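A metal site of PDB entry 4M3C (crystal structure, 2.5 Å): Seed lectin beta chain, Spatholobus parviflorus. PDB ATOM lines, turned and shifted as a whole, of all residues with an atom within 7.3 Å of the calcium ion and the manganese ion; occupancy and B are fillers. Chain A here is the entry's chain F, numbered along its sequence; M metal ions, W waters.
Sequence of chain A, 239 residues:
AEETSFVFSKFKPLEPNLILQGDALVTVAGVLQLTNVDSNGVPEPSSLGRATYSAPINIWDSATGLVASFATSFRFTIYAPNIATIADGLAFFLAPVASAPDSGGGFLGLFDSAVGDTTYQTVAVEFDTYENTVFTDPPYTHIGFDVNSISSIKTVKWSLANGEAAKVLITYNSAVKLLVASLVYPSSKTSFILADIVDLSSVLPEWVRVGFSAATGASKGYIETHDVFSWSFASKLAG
Of the 27 residues printed, 4 come within 4 Å of the calcium ion.
N of Glu 126 is in hydrogen-bond range of O of Gly 144.
A ring nitrogen (ND1) of His 142 is in hydrogen-bond range of the backbone carbonyl oxygen (O) of Tyr 140 (2.9 Å).
The calcium ion is bound by OD2 of Asp 137 (2.3 Å), water W4 (2.3 Å), water W1 (2.4 Å), OD2 of Asp 128 (2.4 Å), O of Tyr 130 (2.5 Å), ND2 of Asn 132 (2.5 Å) and OD1 of Asp 128 (2.5 Å).
OD2 of Asp 128 is bound to the manganese ion.
The manganese ion is bound by OE2 of Glu 126 (2.1 Å).
Water W3 binds the manganese ion, at 2.1 Å.
NE2 of His 142 binds the manganese ion, at 2.2 Å.
The side-chain carboxylate (OD1) of Asp 137 binds the manganese ion, at 2.3 Å.
Water W2 binds the manganese ion, at 2.4 Å.
Water W2 lies within hydrogen-bond range of the side-chain carboxylate (OE1) of Glu 126 and the backbone carbonyl oxygen (O) of Ile 150.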
ATOM      1  N   ASP A  88      30.078 -31.204 -17.413  1.00  0.00           N
ATOM      2  CA  ASP A  88      29.283 -30.314 -16.570  1.00  0.00           C
ATOM      3  C   ASP A  88      30.124 -29.398 -15.690  1.00  0.00           C
ATOM      4  O   ASP A  88      29.661 -28.333 -15.301  1.00  0.00           O
ATOM      5  CB  ASP A  88      28.347 -31.109 -15.651  1.00  0.00           C
ATOM      6  CG  ASP A  88      26.972 -31.328 -16.251  1.00  0.00           C
ATOM      7  OD1 ASP A  88      26.085 -30.461 -16.080  1.00  0.00           O
ATOM      8  OD2 ASP A  88      26.791 -32.390 -16.865  1.00  0.00           O
ATOM      9  N   GLY A  89      31.344 -29.835 -15.353  1.00  0.00           N
ATOM     10  CA  GLY A  89      32.278 -29.013 -14.596  1.00  0.00           C
ATOM     11  C   GLY A  89      33.050 -29.783 -13.526  1.00  0.00           C
ATOM     12  O   GLY A  89      32.938 -30.998 -13.403  1.00  0.00           O
ATOM     13  N   GLY A 105      26.156 -35.291 -13.764  1.00  0.00           N
ATOM     14  CA  GLY A 105      25.620 -34.122 -14.434  1.00  0.00           C
ATOM     15  C   GLY A 105      25.926 -32.847 -13.637  1.00  0.00           C
ATOM     16  O   GLY A 105      27.002 -32.672 -13.067  1.00  0.00           O
ATOM     17  N   GLY A 106      24.941 -31.962 -13.566  1.00  0.00           N
ATOM     18  CA  GLY A 106      25.101 -30.673 -12.925  1.00  0.00           C
ATOM     19  C   GLY A 106      25.254 -30.647 -11.416  1.00  0.00           C
ATOM     20  O   GLY A 106      25.519 -29.591 -10.850  1.00  0.00           O
ATOM     21  N   PHE A 107      25.096 -31.785 -10.751  1.00  0.00           N
ATOM     22  CA  PHE A 107      25.265 -31.804  -9.289  1.00  0.00           C
ATOM     23  C   PHE A 107      26.725 -32.086  -8.971  1.00  0.00           C
ATOM     24  O   PHE A 107      27.128 -31.952  -7.821  1.00  0.00           O
ATOM     25  CB  PHE A 107      24.357 -32.815  -8.557  1.00  0.00           C
ATOM     26  CG  PHE A 107      22.994 -33.018  -9.179  1.00  0.00           C
ATOM     27  CD1 PHE A 107      21.895 -32.317  -8.717  1.00  0.00           C
ATOM     28  CD2 PHE A 107      22.804 -33.947 -10.195  1.00  0.00           C
ATOM     29  CE1 PHE A 107      20.638 -32.530  -9.283  1.00  0.00           C
ATOM     30  CE2 PHE A 107      21.549 -34.173 -10.757  1.00  0.00           C
ATOM     31  CZ  PHE A 107      20.465 -33.458 -10.303  1.00  0.00           C
ATOM     32  N   LEU A 108      27.500 -32.483  -9.995  1.00  0.00           N
ATOM     33  CA  LEU A 108      28.973 -32.579  -9.899  1.00  0.00           C
ATOM     34  C   LEU A 108      29.488 -33.540  -8.818  1.00  0.00           C
ATOM     35  O   LEU A 108      30.490 -33.283  -8.182  1.00  0.00           O
ATOM     36  CB  LEU A 108      29.604 -31.169  -9.686  1.00  0.00           C
ATOM     37  CG  LEU A 108      29.244 -29.862 -10.460  1.00  0.00           C
ATOM     38  CD1 LEU A 108      30.154 -28.684 -10.052  1.00  0.00           C
ATOM     39  CD2 LEU A 108      29.233 -29.943 -11.987  1.00  0.00           C
ATOM     40  N   GLU A 126      32.928 -24.508  -7.151  1.00  0.00           N
ATOM     41  CA  GLU A 126      32.697 -25.167  -8.430  1.00  0.00           C
ATOM     42  C   GLU A 126      33.199 -24.301  -9.594  1.00  0.00           C
ATOM     43  O   GLU A 126      33.256 -23.042  -9.515  1.00  0.00           O
ATOM     44  CB  GLU A 126      31.197 -25.468  -8.628  1.00  0.00           C
ATOM     45  CG  GLU A 126      30.413 -24.173  -8.776  1.00  0.00           C
ATOM     46  CD  GLU A 126      29.023 -24.288  -9.356  1.00  0.00           C
ATOM     47  OE1 GLU A 126      28.183 -25.031  -8.787  1.00  0.00           O
ATOM     48  OE2 GLU A 126      28.751 -23.569 -10.339  1.00  0.00           O
ATOM     49  N   PHE A 127      33.497 -24.996 -10.694  1.00  0.00           N
ATOM     50  CA  PHE A 127      33.931 -24.394 -11.952  1.00  0.00           C
ATOM     51  C   PHE A 127      33.006 -25.015 -12.949  1.00  0.00           C
ATOM     52  O   PHE A 127      33.304 -26.077 -13.536  1.00  0.00           O
ATOM     53  CB  PHE A 127      35.406 -24.734 -12.233  1.00  0.00           C
ATOM     54  CG  PHE A 127      36.345 -24.194 -11.193  1.00  0.00           C
ATOM     55  CD1 PHE A 127      36.925 -22.959 -11.334  1.00  0.00           C
ATOM     56  CD2 PHE A 127      36.595 -24.914 -10.037  1.00  0.00           C
ATOM     57  CE1 PHE A 127      37.757 -22.443 -10.363  1.00  0.00           C
ATOM     58  CE2 PHE A 127      37.426 -24.387  -9.035  1.00  0.00           C
ATOM     59  CZ  PHE A 127      38.013 -23.144  -9.198  1.00  0.00           C
ATOM     60  N   ASP A 128      31.888 -24.314 -13.142  1.00  0.00           N
ATOM     61  CA  ASP A 128      30.720 -24.855 -13.809  1.00  0.00           C
ATOM     62  C   ASP A 128      30.621 -24.559 -15.330  1.00  0.00           C
ATOM     63  O   ASP A 128      30.463 -23.413 -15.749  1.00  0.00           O
ATOM     64  CB  ASP A 128      29.510 -24.303 -13.069  1.00  0.00           C
ATOM     65  CG  ASP A 128      28.223 -24.965 -13.459  1.00  0.00           C
ATOM     66  OD1 ASP A 128      28.100 -25.458 -14.595  1.00  0.00           O
ATOM     67  OD2 ASP A 128      27.296 -24.941 -12.630  1.00  0.00           O
ATOM     68  N   THR A 129      30.670 -25.587 -16.165  1.00  0.00           N
ATOM     69  CA  THR A 129      30.673 -25.298 -17.599  1.00  0.00           C
ATOM     70  C   THR A 129      29.337 -25.384 -18.369  1.00  0.00           C
ATOM     71  O   THR A 129      29.328 -25.248 -19.591  1.00  0.00           O
ATOM     72  CB  THR A 129      31.720 -26.102 -18.344  1.00  0.00           C
ATOM     73  OG1 THR A 129      31.459 -27.498 -18.138  1.00  0.00           O
ATOM     74  CG2 THR A 129      33.110 -25.711 -17.881  1.00  0.00           C
ATOM     75  N   TYR A 130      28.221 -25.582 -17.659  1.00  0.00           N
ATOM     76  CA  TYR A 130      26.940 -25.730 -18.349  1.00  0.00           C
ATOM     77  C   TYR A 130      25.811 -25.136 -17.524  1.00  0.00           C
ATOM     78  O   TYR A 130      25.728 -25.416 -16.328  1.00  0.00           O
ATOM     79  CB  TYR A 130      26.659 -27.222 -18.608  1.00  0.00           C
ATOM     80  CG  TYR A 130      25.255 -27.508 -19.110  1.00  0.00           C
ATOM     81  CD1 TYR A 130      24.956 -27.490 -20.485  1.00  0.00           C
ATOM     82  CD2 TYR A 130      24.236 -27.808 -18.218  1.00  0.00           C
ATOM     83  CE1 TYR A 130      23.674 -27.772 -20.939  1.00  0.00           C
ATOM     84  CE2 TYR A 130      22.942 -28.083 -18.668  1.00  0.00           C
ATOM     85  CZ  TYR A 130      22.659 -28.064 -20.025  1.00  0.00           C
ATOM     86  OH  TYR A 130      21.371 -28.330 -20.475  1.00  0.00           O
ATOM     87  N   GLU A 131      24.942 -24.372 -18.179  1.00  0.00           N
ATOM     88  CA  GLU A 131      23.858 -23.745 -17.469  1.00  0.00           C
ATOM     89  C   GLU A 131      22.678 -24.668 -17.140  1.00  0.00           C
ATOM     90  O   GLU A 131      21.998 -25.188 -18.035  1.00  0.00           O
ATOM     91  CB  GLU A 131      23.313 -22.546 -18.198  1.00  0.00           C
ATOM     92  CG  GLU A 131      22.293 -21.844 -17.328  1.00  0.00           C
ATOM     93  CD  GLU A 131      21.504 -20.808 -18.059  1.00  0.00           C
ATOM     94  OE1 GLU A 131      21.428 -20.854 -19.317  1.00  0.00           O
ATOM     95  OE2 GLU A 131      20.936 -19.944 -17.350  1.00  0.00           O
ATOM     96  N   ASN A 132      22.458 -24.861 -15.841  1.00  0.00           N
ATOM     97  CA  ASN A 132      21.319 -25.612 -15.347  1.00  0.00           C
ATOM     98  C   ASN A 132      20.379 -24.600 -14.738  1.00  0.00           C
ATOM     99  O   ASN A 132      20.628 -24.033 -13.654  1.00  0.00           O
ATOM    100  CB  ASN A 132      21.750 -26.638 -14.287  1.00  0.00           C
ATOM    101  CG  ASN A 132      22.627 -27.752 -14.862  1.00  0.00           C
ATOM    102  OD1 ASN A 132      22.146 -28.853 -15.117  1.00  0.00           O
ATOM    103  ND2 ASN A 132      23.924 -27.466 -15.047  1.00  0.00           N
ATOM    104  N   THR A 133      19.290 -24.347 -15.464  1.00  0.00           N
ATOM    105  CA  THR A 133      18.323 -23.362 -15.022  1.00  0.00           C
ATOM    106  C   THR A 133      17.676 -23.803 -13.720  1.00  0.00           C
ATOM    107  O   THR A 133      17.379 -22.974 -12.856  1.00  0.00           O
ATOM    108  CB  THR A 133      17.266 -23.099 -16.104  1.00  0.00           C
ATOM    109  OG1 THR A 133      16.941 -24.340 -16.760  1.00  0.00           O
ATOM    110  CG2 THR A 133      17.800 -22.113 -17.139  1.00  0.00           C
ATOM    111  N   PHE A 135      18.985 -25.102 -11.248  1.00  0.00           N
ATOM    112  CA  PHE A 135      19.873 -24.685 -10.151  1.00  0.00           C
ATOM    113  C   PHE A 135      20.117 -23.176 -10.123  1.00  0.00           C
ATOM    114  O   PHE A 135      21.025 -22.681  -9.443  1.00  0.00           O
ATOM    115  CB  PHE A 135      21.215 -25.371 -10.267  1.00  0.00           C
ATOM    116  CG  PHE A 135      21.147 -26.847 -10.460  1.00  0.00           C
ATOM    117  CD1 PHE A 135      20.029 -27.585 -10.064  1.00  0.00           C
ATOM    118  CD2 PHE A 135      22.230 -27.524 -10.995  1.00  0.00           C
ATOM    119  CE1 PHE A 135      20.000 -28.968 -10.243  1.00  0.00           C
ATOM    120  CE2 PHE A 135      22.206 -28.898 -11.174  1.00  0.00           C
ATOM    121  CZ  PHE A 135      21.093 -29.615 -10.805  1.00  0.00           C
ATOM    122  N   THR A 136      19.297 -22.454 -10.868  1.00  0.00           N
ATOM    123  CA  THR A 136      19.501 -21.009 -11.106  1.00  0.00           C
ATOM    124  C   THR A 136      20.966 -20.603 -11.441  1.00  0.00           C
ATOM    125  O   THR A 136      21.478 -19.623 -10.904  1.00  0.00           O
ATOM    126  CB  THR A 136      18.698 -20.119 -10.070  1.00  0.00           C
ATOM    127  OG1 THR A 136      19.184 -18.766 -10.062  1.00  0.00           O
ATOM    128  CG2 THR A 136      18.667 -20.698  -8.633  1.00  0.00           C
ATOM    129  N   ASP A 137      21.598 -21.363 -12.345  1.00  0.00           N
ATOM    130  CA  ASP A 137      22.906 -21.052 -12.983  1.00  0.00           C
ATOM    131  C   ASP A 137      22.833 -19.797 -13.843  1.00  0.00           C
ATOM    132  O   ASP A 137      21.854 -19.568 -14.530  1.00  0.00           O
ATOM    133  CB  ASP A 137      23.351 -22.202 -13.909  1.00  0.00           C
ATOM    134  CG  ASP A 137      24.208 -23.245 -13.223  1.00  0.00           C
ATOM    135  OD1 ASP A 137      24.845 -22.927 -12.198  1.00  0.00           O
ATOM    136  OD2 ASP A 137      24.308 -24.396 -13.708  1.00  0.00           O
ATOM    137  N   PRO A 138      23.906 -18.990 -13.867  1.00  0.00           N
ATOM    138  CA  PRO A 138      23.859 -17.823 -14.768  1.00  0.00           C
ATOM    139  C   PRO A 138      24.075 -18.231 -16.236  1.00  0.00           C
ATOM    140  O   PRO A 138      24.575 -19.334 -16.492  1.00  0.00           O
ATOM    141  CB  PRO A 138      25.005 -16.930 -14.251  1.00  0.00           C
ATOM    142  CG  PRO A 138      25.902 -17.834 -13.471  1.00  0.00           C
ATOM    143  CD  PRO A 138      25.161 -19.078 -13.085  1.00  0.00           C
ATOM    144  N   TYR A 140      26.287 -18.056 -18.418  1.00  0.00           N
ATOM    145  CA  TYR A 140      27.683 -18.080 -18.844  1.00  0.00           C
ATOM    146  C   TYR A 140      28.428 -19.044 -17.959  1.00  0.00           C
ATOM    147  O   TYR A 140      28.019 -19.266 -16.814  1.00  0.00           O
ATOM    148  CB  TYR A 140      28.336 -16.694 -18.786  1.00  0.00           C
ATOM    149  CG  TYR A 140      28.021 -15.895 -17.563  1.00  0.00           C
ATOM    150  CD1 TYR A 140      28.574 -16.229 -16.338  1.00  0.00           C
ATOM    151  CD2 TYR A 140      27.171 -14.774 -17.623  1.00  0.00           C
ATOM    152  CE1 TYR A 140      28.280 -15.514 -15.185  1.00  0.00           C
ATOM    153  CE2 TYR A 140      26.873 -14.033 -16.479  1.00  0.00           C
ATOM    154  CZ  TYR A 140      27.425 -14.401 -15.245  1.00  0.00           C
ATOM    155  OH  TYR A 140      27.183 -13.709 -14.070  1.00  0.00           O
ATOM    156  N   HIS A 142      30.862 -20.359 -15.229  1.00  0.00           N
ATOM    157  CA  HIS A 142      31.103 -19.575 -14.005  1.00  0.00           C
ATOM    158  C   HIS A 142      31.844 -20.277 -12.924  1.00  0.00           C
ATOM    159  O   HIS A 142      31.841 -21.516 -12.822  1.00  0.00           O
ATOM    160  CB  HIS A 142      29.785 -19.069 -13.432  1.00  0.00           C
ATOM    161  CG  HIS A 142      28.771 -20.155 -13.261  1.00  0.00           C
ATOM    162  ND1 HIS A 142      27.979 -20.564 -14.267  1.00  0.00           N
ATOM    163  CD2 HIS A 142      28.482 -20.990 -12.174  1.00  0.00           C
ATOM    164  CE1 HIS A 142      27.219 -21.594 -13.849  1.00  0.00           C
ATOM    165  NE2 HIS A 142      27.528 -21.854 -12.559  1.00  0.00           N
ATOM    166  N   ILE A 143      32.497 -19.453 -12.099  1.00  0.00           N
ATOM    167  CA  ILE A 143      33.018 -19.851 -10.790  1.00  0.00           C
ATOM    168  C   ILE A 143      31.944 -19.547  -9.759  1.00  0.00           C
ATOM    169  O   ILE A 143      31.265 -18.535  -9.852  1.00  0.00           O
ATOM    170  CB  ILE A 143      34.283 -19.055 -10.439  1.00  0.00           C
ATOM    171  CG1 ILE A 143      35.369 -19.367 -11.473  1.00  0.00           C
ATOM    172  CG2 ILE A 143      34.779 -19.427  -9.047  1.00  0.00           C
ATOM    173  CD1 ILE A 143      36.645 -18.577 -11.266  1.00  0.00           C
ATOM    174  N   GLY A 144      31.796 -20.411  -8.767  1.00  0.00           N
ATOM    175  CA  GLY A 144      30.749 -20.255  -7.759  1.00  0.00           C
ATOM    176  C   GLY A 144      31.127 -20.918  -6.454  1.00  0.00           C
ATOM    177  O   GLY A 144      31.995 -21.800  -6.433  1.00  0.00           O
ATOM    178  N   ASP A 146      29.529 -23.101  -3.394  1.00  0.00           N
ATOM    179  CA  ASP A 146      28.425 -23.979  -3.052  1.00  0.00           C
ATOM    180  C   ASP A 146      28.489 -24.288  -1.533  1.00  0.00           C
ATOM    181  O   ASP A 146      29.524 -24.776  -1.017  1.00  0.00           O
ATOM    182  CB  ASP A 146      28.527 -25.254  -3.880  1.00  0.00           C
ATOM    183  CG  ASP A 146      28.337 -25.007  -5.373  1.00  0.00           C
ATOM    184  OD1 ASP A 146      28.014 -23.850  -5.784  1.00  0.00           O
ATOM    185  OD2 ASP A 146      28.501 -25.990  -6.153  1.00  0.00           O
ATOM    186  N   ILE A 150      23.685 -27.007  -4.585  1.00  0.00           N
ATOM    187  CA  ILE A 150      24.266 -26.678  -5.897  1.00  0.00           C
ATOM    188  C   ILE A 150      23.837 -25.248  -6.373  1.00  0.00           C
ATOM    189  O   ILE A 150      24.272 -24.759  -7.400  1.00  0.00           O
ATOM    190  CB  ILE A 150      23.941 -27.756  -6.959  1.00  0.00           C
ATOM    191  CG1 ILE A 150      24.842 -27.623  -8.182  1.00  0.00           C
ATOM    192  CG2 ILE A 150      22.486 -27.689  -7.371  1.00  0.00           C
ATOM    193  CD1 ILE A 150      26.208 -28.223  -8.012  1.00  0.00           C
ATOM    194  N   SER A 151      22.982 -24.568  -5.623  1.00  0.00           N
ATOM    195  CA  SER A 151      22.594 -23.250  -6.045  1.00  0.00           C
ATOM    196  C   SER A 151      23.553 -22.287  -5.352  1.00  0.00           C
ATOM    197  O   SER A 151      23.382 -21.974  -4.180  1.00  0.00           O
ATOM    198  CB  SER A 151      21.138 -22.995  -5.672  1.00  0.00           C
ATOM    199  OG  SER A 151      20.630 -21.809  -6.287  1.00  0.00           O
ATOM    200  N   SER A 152      24.582 -21.854  -6.071  1.00  0.00           N
ATOM    201  CA  SER A 152      25.669 -21.115  -5.457  1.00  0.00           C
ATOM    202  C   SER A 152      25.174 -19.931  -4.646  1.00  0.00           C
ATOM    203  O   SER A 152      24.324 -19.218  -5.138  1.00  0.00           O
ATOM    204  CB  SER A 152      26.599 -20.611  -6.546  1.00  0.00           C
ATOM    205  OG  SER A 152      27.006 -21.655  -7.395  1.00  0.00           O
ATOM    206  N   THR A 155      28.435 -16.242  -7.497  1.00  0.00           N
ATOM    207  CA  THR A 155      29.190 -16.587  -8.684  1.00  0.00           C
ATOM    208  C   THR A 155      29.819 -15.326  -9.293  1.00  0.00           C
ATOM    209  O   THR A 155      29.488 -14.204  -8.902  1.00  0.00           O
ATOM    210  CB  THR A 155      28.281 -17.193  -9.770  1.00  0.00           C
ATOM    211  OG1 THR A 155      27.410 -16.180 -10.304  1.00  0.00           O
ATOM    212  CG2 THR A 155      27.446 -18.367  -9.220  1.00  0.00           C
HETATM  213 CA    CA M   1      25.736 -26.169 -13.989  1.00  0.00          CA
HETATM  214 MN    MN M   2      26.820 -23.472 -11.214  1.00  0.00          MN
HETATM  215  O   HOH W   1      25.409 -27.085 -11.801  1.00  0.00           O
HETATM  216  O   HOH W   2      25.687 -25.101  -9.844  1.00  0.00           O
HETATM  217  O   HOH W   3      26.145 -22.173  -9.672  1.00  0.00           O
HETATM  218  O   HOH W   4      26.943 -27.981 -14.770  1.00  0.00           O
